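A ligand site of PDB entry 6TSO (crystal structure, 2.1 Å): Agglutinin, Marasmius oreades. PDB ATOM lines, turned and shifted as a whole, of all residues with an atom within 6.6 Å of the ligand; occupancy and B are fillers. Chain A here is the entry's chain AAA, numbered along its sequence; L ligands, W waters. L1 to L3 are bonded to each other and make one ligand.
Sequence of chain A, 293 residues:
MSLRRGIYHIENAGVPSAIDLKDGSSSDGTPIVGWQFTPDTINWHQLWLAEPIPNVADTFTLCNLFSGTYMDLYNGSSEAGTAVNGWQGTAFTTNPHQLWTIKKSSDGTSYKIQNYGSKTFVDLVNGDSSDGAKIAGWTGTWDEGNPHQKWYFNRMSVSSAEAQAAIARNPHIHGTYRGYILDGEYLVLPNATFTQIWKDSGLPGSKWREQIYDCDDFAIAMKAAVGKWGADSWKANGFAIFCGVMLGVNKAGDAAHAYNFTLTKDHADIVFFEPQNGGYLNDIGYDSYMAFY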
ATOM      1  N   HIS A   9       6.280 -17.434  -0.445  1.00  0.00           N
ATOM      2  CA  HIS A   9       5.802 -18.737   0.078  1.00  0.00           C
ATOM      3  C   HIS A   9       6.447 -19.779  -0.827  1.00  0.00           C
ATOM      4  O   HIS A   9       6.139 -19.766  -2.045  1.00  0.00           O
ATOM      5  CB  HIS A   9       4.275 -18.738   0.150  1.00  0.00           C
ATOM      6  CG  HIS A   9       3.706 -19.882   0.895  1.00  0.00           C
ATOM      7  ND1 HIS A   9       2.969 -20.864   0.269  1.00  0.00           N
ATOM      8  CD2 HIS A   9       3.796 -20.235   2.206  1.00  0.00           C
ATOM      9  CE1 HIS A   9       2.609 -21.766   1.168  1.00  0.00           C
ATOM     10  NE2 HIS A   9       3.125 -21.403   2.370  1.00  0.00           N
ATOM     11  N   ASP A  20       8.945 -24.477   5.885  1.00  0.00           N
ATOM     12  CA  ASP A  20       8.287 -24.111   7.147  1.00  0.00           C
ATOM     13  C   ASP A  20       9.357 -24.187   8.235  1.00  0.00           C
ATOM     14  O   ASP A  20      10.024 -25.208   8.357  1.00  0.00           O
ATOM     15  CB  ASP A  20       7.065 -25.016   7.365  1.00  0.00           C
ATOM     16  CG  ASP A  20       6.297 -24.790   8.650  1.00  0.00           C
ATOM     17  OD1 ASP A  20       6.895 -24.955   9.759  1.00  0.00           O
ATOM     18  OD2 ASP A  20       5.100 -24.477   8.550  1.00  0.00           O
ATOM     19  N   LEU A  21       9.559 -23.116   8.979  1.00  0.00           N
ATOM     20  CA  LEU A  21      10.455 -23.129  10.144  1.00  0.00           C
ATOM     21  C   LEU A  21       9.611 -23.627  11.303  1.00  0.00           C
ATOM     22  O   LEU A  21       8.628 -22.971  11.669  1.00  0.00           O
ATOM     23  CB  LEU A  21      10.988 -21.715  10.341  1.00  0.00           C
ATOM     24  CG  LEU A  21      11.822 -21.517  11.587  1.00  0.00           C
ATOM     25  CD1 LEU A  21      13.149 -22.266  11.493  1.00  0.00           C
ATOM     26  CD2 LEU A  21      12.069 -20.032  11.808  1.00  0.00           C
ATOM     27  N   LYS A  22       9.948 -24.801  11.826  1.00  0.00           N
ATOM     28  CA  LYS A  22       9.012 -25.571  12.694  1.00  0.00           C
ATOM     29  C   LYS A  22       8.624 -24.693  13.905  1.00  0.00           C
ATOM     30  O   LYS A  22       9.519 -24.193  14.588  1.00  0.00           O
ATOM     31  CB  LYS A  22       9.674 -26.888  13.085  1.00  0.00           C
ATOM     32  CG  LYS A  22       8.638 -27.956  13.383  1.00  0.00           C
ATOM     33  CD  LYS A  22       9.180 -29.312  13.680  1.00  0.00           C
ATOM     34  CE  LYS A  22       8.078 -30.168  14.260  1.00  0.00           C
ATOM     35  NZ  LYS A  22       8.578 -31.502  14.646  1.00  0.00           N
ATOM     36  N   ASP A  23       7.330 -24.516  14.131  1.00  0.00           N
ATOM     37  CA  ASP A  23       6.720 -23.739  15.262  1.00  0.00           C
ATOM     38  C   ASP A  23       7.169 -22.278  15.186  1.00  0.00           C
ATOM     39  O   ASP A  23       6.939 -21.530  16.147  1.00  0.00           O
ATOM     40  CB  ASP A  23       7.048 -24.348  16.628  1.00  0.00           C
ATOM     41  CG  ASP A  23       6.047 -24.001  17.729  1.00  0.00           C
ATOM     42  OD1 ASP A  23       4.826 -24.057  17.469  1.00  0.00           O
ATOM     43  OD2 ASP A  23       6.491 -23.651  18.849  1.00  0.00           O
ATOM     44  N   GLY A  24       7.719 -21.820  14.064  1.00  0.00           N
ATOM     45  CA  GLY A  24       8.181 -20.439  13.906  1.00  0.00           C
ATOM     46  C   GLY A  24       9.252 -20.079  14.929  1.00  0.00           C
ATOM     47  O   GLY A  24       9.462 -18.856  15.149  1.00  0.00           O
ATOM     48  N   VAL A  33      11.311 -27.584   7.663  1.00  0.00           N
ATOM     49  CA  VAL A  33      10.678 -28.864   7.243  1.00  0.00           C
ATOM     50  C   VAL A  33       9.616 -28.552   6.194  1.00  0.00           C
ATOM     51  O   VAL A  33       9.197 -27.383   6.079  1.00  0.00           O
ATOM     52  CB  VAL A  33      10.081 -29.596   8.461  1.00  0.00           C
ATOM     53  CG1 VAL A  33      11.142 -29.908   9.511  1.00  0.00           C
ATOM     54  CG2 VAL A  33       8.935 -28.825   9.104  1.00  0.00           C
ATOM     55  N   TRP A  35       5.709 -28.705   5.209  1.00  0.00           N
ATOM     56  CA  TRP A  35       4.423 -28.631   5.920  1.00  0.00           C
ATOM     57  C   TRP A  35       3.352 -28.202   4.929  1.00  0.00           C
ATOM     58  O   TRP A  35       3.677 -27.416   4.035  1.00  0.00           O
ATOM     59  CB  TRP A  35       4.514 -27.675   7.130  1.00  0.00           C
ATOM     60  CG  TRP A  35       3.629 -28.049   8.263  1.00  0.00           C
ATOM     61  CD1 TRP A  35       2.278 -27.851   8.371  1.00  0.00           C
ATOM     62  CD2 TRP A  35       4.028 -28.742   9.473  1.00  0.00           C
ATOM     63  NE1 TRP A  35       1.821 -28.308   9.584  1.00  0.00           N
ATOM     64  CE2 TRP A  35       2.861 -28.898  10.256  1.00  0.00           C
ATOM     65  CE3 TRP A  35       5.250 -29.183   9.987  1.00  0.00           C
ATOM     66  CZ2 TRP A  35       2.889 -29.530  11.503  1.00  0.00           C
ATOM     67  CZ3 TRP A  35       5.268 -29.788  11.225  1.00  0.00           C
ATOM     68  CH2 TRP A  35       4.106 -29.928  11.983  1.00  0.00           C
ATOM     69  N   GLN A  36       2.136 -28.711   5.070  1.00  0.00           N
ATOM     70  CA  GLN A  36       0.996 -28.322   4.207  1.00  0.00           C
ATOM     71  C   GLN A  36       0.634 -26.873   4.538  1.00  0.00           C
ATOM     72  O   GLN A  36       1.081 -26.346   5.554  1.00  0.00           O
ATOM     73  CB  GLN A  36      -0.210 -29.261   4.408  1.00  0.00           C
ATOM     74  CG  GLN A  36      -0.768 -29.238   5.811  1.00  0.00           C
ATOM     75  CD  GLN A  36      -1.904 -30.217   5.942  1.00  0.00           C
ATOM     76  OE1 GLN A  36      -2.891 -30.117   5.205  1.00  0.00           O
ATOM     77  NE2 GLN A  36      -1.720 -31.213   6.818  1.00  0.00           N
ATOM     78  N   PHE A  37      -0.174 -26.246   3.695  1.00  0.00           N
ATOM     79  CA  PHE A  37      -0.497 -24.822   3.816  1.00  0.00           C
ATOM     80  C   PHE A  37      -1.920 -24.590   3.336  1.00  0.00           C
ATOM     81  O   PHE A  37      -2.516 -25.497   2.748  1.00  0.00           O
ATOM     82  CB  PHE A  37       0.553 -24.056   2.991  1.00  0.00           C
ATOM     83  CG  PHE A  37       0.637 -24.478   1.560  1.00  0.00           C
ATOM     84  CD1 PHE A  37      -0.113 -23.839   0.593  1.00  0.00           C
ATOM     85  CD2 PHE A  37       1.590 -25.405   1.165  1.00  0.00           C
ATOM     86  CE1 PHE A  37       0.016 -24.193  -0.740  1.00  0.00           C
ATOM     87  CE2 PHE A  37       1.741 -25.738  -0.175  1.00  0.00           C
ATOM     88  CZ  PHE A  37       0.937 -25.145  -1.121  1.00  0.00           C
ATOM     89  N   THR A  38      -2.453 -23.406   3.625  1.00  0.00           N
ATOM     90  CA  THR A  38      -3.815 -23.017   3.195  1.00  0.00           C
ATOM     91  C   THR A  38      -3.605 -21.802   2.292  1.00  0.00           C
ATOM     92  O   THR A  38      -3.028 -20.819   2.722  1.00  0.00           O
ATOM     93  CB  THR A  38      -4.747 -22.764   4.381  1.00  0.00           C
ATOM     94  OG1 THR A  38      -4.571 -23.765   5.383  1.00  0.00           O
ATOM     95  CG2 THR A  38      -6.211 -22.785   4.001  1.00  0.00           C
ATOM     96  N   PRO A  39      -4.051 -21.854   1.020  1.00  0.00           N
ATOM     97  CA  PRO A  39      -4.030 -20.682   0.150  1.00  0.00           C
ATOM     98  C   PRO A  39      -4.835 -19.510   0.735  1.00  0.00           C
ATOM     99  O   PRO A  39      -5.749 -19.780   1.474  1.00  0.00           O
ATOM    100  CB  PRO A  39      -4.714 -21.149  -1.149  1.00  0.00           C
ATOM    101  CG  PRO A  39      -4.633 -22.666  -1.088  1.00  0.00           C
ATOM    102  CD  PRO A  39      -4.684 -23.012   0.390  1.00  0.00           C
ATOM    103  N   THR A  41      -4.343 -17.378   2.958  1.00  0.00           N
ATOM    104  CA  THR A  41      -4.130 -17.123   4.392  1.00  0.00           C
ATOM    105  C   THR A  41      -2.722 -16.564   4.569  1.00  0.00           C
ATOM    106  O   THR A  41      -1.906 -16.597   3.613  1.00  0.00           O
ATOM    107  CB  THR A  41      -4.287 -18.361   5.291  1.00  0.00           C
ATOM    108  OG1 THR A  41      -3.286 -19.348   4.976  1.00  0.00           O
ATOM    109  CG2 THR A  41      -5.662 -19.008   5.174  1.00  0.00           C
ATOM    110  N   ILE A  42      -2.460 -16.062   5.771  1.00  0.00           N
ATOM    111  CA  ILE A  42      -1.094 -15.856   6.305  1.00  0.00           C
ATOM    112  C   ILE A  42      -0.615 -17.215   6.790  1.00  0.00           C
ATOM    113  O   ILE A  42      -1.234 -17.725   7.736  1.00  0.00           O
ATOM    114  CB  ILE A  42      -1.110 -14.779   7.414  1.00  0.00           C
ATOM    115  CG1 ILE A  42      -1.527 -13.414   6.838  1.00  0.00           C
ATOM    116  CG2 ILE A  42       0.221 -14.728   8.144  1.00  0.00           C
ATOM    117  CD1 ILE A  42      -0.786 -13.010   5.565  1.00  0.00           C
ATOM    118  N   ASN A  43       0.342 -17.842   6.080  1.00  0.00           N
ATOM    119  CA  ASN A  43       1.006 -19.092   6.537  1.00  0.00           C
ATOM    120  C   ASN A  43       2.186 -18.644   7.422  1.00  0.00           C
ATOM    121  O   ASN A  43       3.276 -18.376   6.906  1.00  0.00           O
ATOM    122  CB  ASN A  43       1.370 -19.973   5.343  1.00  0.00           C
ATOM    123  CG  ASN A  43       0.118 -20.532   4.709  1.00  0.00           C
ATOM    124  OD1 ASN A  43      -0.520 -21.381   5.325  1.00  0.00           O
ATOM    125  ND2 ASN A  43      -0.232 -20.061   3.515  1.00  0.00           N
ATOM    126  N   TRP A  44       1.875 -18.466   8.695  1.00  0.00           N
ATOM    127  CA  TRP A  44       2.683 -17.723   9.699  1.00  0.00           C
ATOM    128  C   TRP A  44       4.152 -18.190   9.770  1.00  0.00           C
ATOM    129  O   TRP A  44       5.023 -17.316  10.059  1.00  0.00           O
ATOM    130  CB  TRP A  44       2.027 -17.855  11.072  1.00  0.00           C
ATOM    131  CG  TRP A  44       0.907 -16.875  11.241  1.00  0.00           C
ATOM    132  CD1 TRP A  44      -0.421 -17.116  11.085  1.00  0.00           C
ATOM    133  CD2 TRP A  44       1.039 -15.458  11.482  1.00  0.00           C
ATOM    134  NE1 TRP A  44      -1.122 -15.960  11.265  1.00  0.00           N
ATOM    135  CE2 TRP A  44      -0.259 -14.931  11.505  1.00  0.00           C
ATOM    136  CE3 TRP A  44       2.128 -14.624  11.729  1.00  0.00           C
ATOM    137  CZ2 TRP A  44      -0.507 -13.586  11.769  1.00  0.00           C
ATOM    138  CZ3 TRP A  44       1.884 -13.291  11.975  1.00  0.00           C
ATOM    139  CH2 TRP A  44       0.588 -12.773  11.993  1.00  0.00           C
ATOM    140  N   HIS A  45       4.436 -19.477   9.559  1.00  0.00           N
ATOM    141  CA  HIS A  45       5.836 -19.981   9.713  1.00  0.00           C
ATOM    142  C   HIS A  45       6.498 -20.224   8.361  1.00  0.00           C
ATOM    143  O   HIS A  45       7.616 -20.779   8.369  1.00  0.00           O
ATOM    144  CB  HIS A  45       5.830 -21.258  10.546  1.00  0.00           C
ATOM    145  CG  HIS A  45       5.180 -21.061  11.860  1.00  0.00           C
ATOM    146  ND1 HIS A  45       4.696 -22.126  12.576  1.00  0.00           N
ATOM    147  CD2 HIS A  45       4.959 -19.953  12.603  1.00  0.00           C
ATOM    148  CE1 HIS A  45       4.202 -21.679  13.728  1.00  0.00           C
ATOM    149  NE2 HIS A  45       4.354 -20.354  13.773  1.00  0.00           N
ATOM    150  N   GLN A  46       5.862 -19.793   7.265  1.00  0.00           N
ATOM    151  CA  GLN A  46       6.200 -20.292   5.907  1.00  0.00           C
ATOM    152  C   GLN A  46       6.493 -19.096   4.962  1.00  0.00           C
ATOM    153  O   GLN A  46       6.504 -19.336   3.759  1.00  0.00           O
ATOM    154  CB  GLN A  46       5.048 -21.182   5.412  1.00  0.00           C
ATOM    155  CG  GLN A  46       4.785 -22.458   6.243  1.00  0.00           C
ATOM    156  CD  GLN A  46       3.575 -23.244   5.752  1.00  0.00           C
ATOM    157  OE1 GLN A  46       2.930 -22.845   4.789  1.00  0.00           O
ATOM    158  NE2 GLN A  46       3.259 -24.376   6.376  1.00  0.00           N
ATOM    159  N   PHE A  66       8.509 -14.322  10.300  1.00  0.00           N
ATOM    160  CA  PHE A  66       8.030 -14.532  11.684  1.00  0.00           C
ATOM    161  C   PHE A  66       9.198 -14.541  12.689  1.00  0.00           C
ATOM    162  O   PHE A  66       9.121 -13.831  13.704  1.00  0.00           O
ATOM    163  CB  PHE A  66       7.291 -15.865  11.829  1.00  0.00           C
ATOM    164  CG  PHE A  66       6.612 -15.977  13.162  1.00  0.00           C
ATOM    165  CD1 PHE A  66       5.629 -15.076  13.511  1.00  0.00           C
ATOM    166  CD2 PHE A  66       6.993 -16.943  14.070  1.00  0.00           C
ATOM    167  CE1 PHE A  66       5.000 -15.152  14.757  1.00  0.00           C
ATOM    168  CE2 PHE A  66       6.376 -17.036  15.308  1.00  0.00           C
ATOM    169  CZ  PHE A  66       5.391 -16.127  15.662  1.00  0.00           C
ATOM    170  N   ASP A 131       3.656 -33.711   7.057  1.00  0.00           N
ATOM    171  CA  ASP A 131       3.902 -32.507   7.890  1.00  0.00           C
ATOM    172  C   ASP A 131       5.093 -32.766   8.807  1.00  0.00           C
ATOM    173  O   ASP A 131       4.960 -33.652   9.652  1.00  0.00           O
ATOM    174  CB  ASP A 131       2.660 -32.153   8.697  1.00  0.00           C
ATOM    175  CG  ASP A 131       1.560 -31.573   7.840  1.00  0.00           C
ATOM    176  OD1 ASP A 131       1.885 -31.079   6.744  1.00  0.00           O
ATOM    177  OD2 ASP A 131       0.380 -31.582   8.283  1.00  0.00           O
HETATM  178  C1  LIG L   1      -0.957 -22.669  12.226  1.00  0.00           C
HETATM  179  C2  LIG L   1      -2.370 -22.837  12.788  1.00  0.00           C
HETATM  180  C3  LIG L   1      -2.357 -22.560  14.279  1.00  0.00           C
HETATM  181  C4  LIG L   1      -1.762 -21.205  14.536  1.00  0.00           C
HETATM  182  C5  LIG L   1      -0.354 -21.146  13.978  1.00  0.00           C
HETATM  183  C6  LIG L   1       0.314 -19.790  14.095  1.00  0.00           C
HETATM  184  O1  LIG L   1      -2.813 -24.161  12.485  1.00  0.00           O
HETATM  185  O2  LIG L   1      -3.684 -22.585  14.743  1.00  0.00           O
HETATM  186  O3  LIG L   1      -2.503 -20.159  13.880  1.00  0.00           O
HETATM  187  O4  LIG L   1      -0.390 -21.399  12.580  1.00  0.00           O
HETATM  188  C1  LG2 L   2       1.879 -24.602  13.459  1.00  0.00           C
HETATM  189  C2  LG2 L   2       1.178 -23.866  12.300  1.00  0.00           C
HETATM  190  C3  LG2 L   2       1.284 -24.650  10.996  1.00  0.00           C
HETATM  191  C4  LG2 L   2       2.759 -25.013  10.787  1.00  0.00           C
HETATM  192  C5  LG2 L   2       3.350 -25.730  12.019  1.00  0.00           C
HETATM  193  C6  LG2 L   2       4.837 -25.980  11.822  1.00  0.00           C
HETATM  194  O1  LG2 L   2       1.954 -23.665  14.476  1.00  0.00           O
HETATM  195  O2  LG2 L   2      -0.173 -23.661  12.721  1.00  0.00           O
HETATM  196  O3  LG2 L   2       0.776 -23.944   9.808  1.00  0.00           O
HETATM  197  O4  LG2 L   2       3.494 -23.804  10.470  1.00  0.00           O
HETATM  198  O5  LG2 L   2       3.223 -24.971  13.197  1.00  0.00           O
HETATM  199  O6  LG2 L   2       5.563 -24.747  12.029  1.00  0.00           O
HETATM  200  C1  LG3 L   3       0.558 -24.596   8.677  1.00  0.00           C
HETATM  201  C2  LG3 L   3      -0.177 -23.683   7.666  1.00  0.00           C
HETATM  202  C3  LG3 L   3      -1.710 -23.735   7.824  1.00  0.00           C
HETATM  203  C4  LG3 L   3      -2.179 -25.175   7.980  1.00  0.00           C
HETATM  204  C5  LG3 L   3      -1.413 -25.835   9.151  1.00  0.00           C
HETATM  205  C6  LG3 L   3      -1.878 -27.222   9.459  1.00  0.00           C
HETATM  206  O1  LG3 L   3       0.277 -22.332   7.822  1.00  0.00           O
HETATM  207  O2  LG3 L   3      -2.287 -23.054   6.679  1.00  0.00           O
HETATM  208  O3  LG3 L   3      -1.982 -25.868   6.750  1.00  0.00           O
HETATM  209  O4  LG3 L   3      -0.058 -25.885   8.765  1.00  0.00           O
HETATM  210  O5  LG3 L   3      -1.009 -27.883  10.400  1.00  0.00           O
HETATM  211  O   HOH W   1      -1.644 -26.546  12.986  1.00  0.00           O
HETATM  212  O   HOH W   2       4.119 -25.990  15.683  1.00  0.00           O
HETATM  213  O   HOH W   3      -0.489 -20.085   9.680  1.00  0.00           O
HETATM  214  O   HOH W   4      -2.615 -20.563   7.322  1.00  0.00           O
HETATM  215  O   HOH W   5       2.470 -21.775   8.970  1.00  0.00           O
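A ring nitrogen (ND1) of His 45 lies within hydrogen-bond range of the backbone NH (N) of Gly 24 (3.4 Å). The side-chain hydroxyl of Thr 41 sits at hydrogen-bond distance from the side-chain amide oxygen of Asn 43, at 3.5 Å. O of Thr 38 is in hydrogen-bond range of OG1 of Thr 41. N of Val 33 sits at hydrogen-bond distance from O of Asp 20, at 2.8 Å. NE2 of Gln 36 sits at hydrogen-bond distance from OD2 of Asp 131, 2.6 Å away. The side-chain amide nitrogen of Gln 46 is in hydrogen-bond range of the backbone carbonyl oxygen of Gln 36 (3.0 Å). The backbone carbonyl oxygen (O) of His 45 is in hydrogen-bond range of the backbone NH (N) of Leu 21 (3.1 Å). The side-chain amide oxygen (OE1) of Gln 46 lies within hydrogen-bond range of a ring nitrogen (NE2) of His 9 (2.8 Å).
O6 of LG2 L2 is in hydrogen-bond range of N of Asp 23 (2.8 Å). O2 of LG3 L3 sits at hydrogen-bond distance from OG1 of Thr 38, at 2.7 Å. OD1 of Asn 43 sits at hydrogen-bond distance from O2 of LG3 L3 (2.8 Å). NE1 of Trp 35 sits at hydrogen-bond distance from O5 of LG3 L3, at 3.0 Å. A ring nitrogen (ND1) of His 45 lies within hydrogen-bond range of an oxygen (O6) of LG2 L2 (2.8 Å). O of Gln 36 lies within hydrogen-bond range of O3 of LG3 L3, at 3.3 Å. An oxygen (O2) of LG3 L3 sits at hydrogen-bond distance from the backbone NH (N) of Thr 38, 3.1 Å away. OD2 of Asp 20 is in hydrogen-bond range of O4 of LG2 L2 (2.6 Å).
Water W5 lies within hydrogen-bond range of O1 of LG3 L3 (2.5 Å), N of His 45 (3.1 Å) and N of Trp 44 (3.4 Å). Water W4 lies within hydrogen-bond range of O2 of LG3 L3 (2.6 Å), OG1 of Thr 41 (2.7 Å), OD1 of Asn 43 (3.0 Å) and O of Ile 42 (3.2 Å). Water W2 bridges OD1 of Asp 23 and O5 of LG2 L2. Water W3 lies within hydrogen-bond range of O1 of LG3 L3 (3.0 Å), N of Trp 44 (3.0 Å) and O of Ile 42 (3.1 Å).
Residues that only touch the ligand: Phe 37, Gln 46, Leu 21, Lys 22 and Trp 44. 12 residues have an atom within 4 Å of the ligand: Asp 20, Leu 21, Lys 22, Asp 23, Trp 35, Gln 36, Phe 37, Thr 38, Asn 43, Trp 44, His 45 and Gln 46. Along chain A the residues within 4 Å of the ligand span positions 20 to 46. The nearest printed residue that does not touch the ligand is Gly 24 (4.2 Å).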
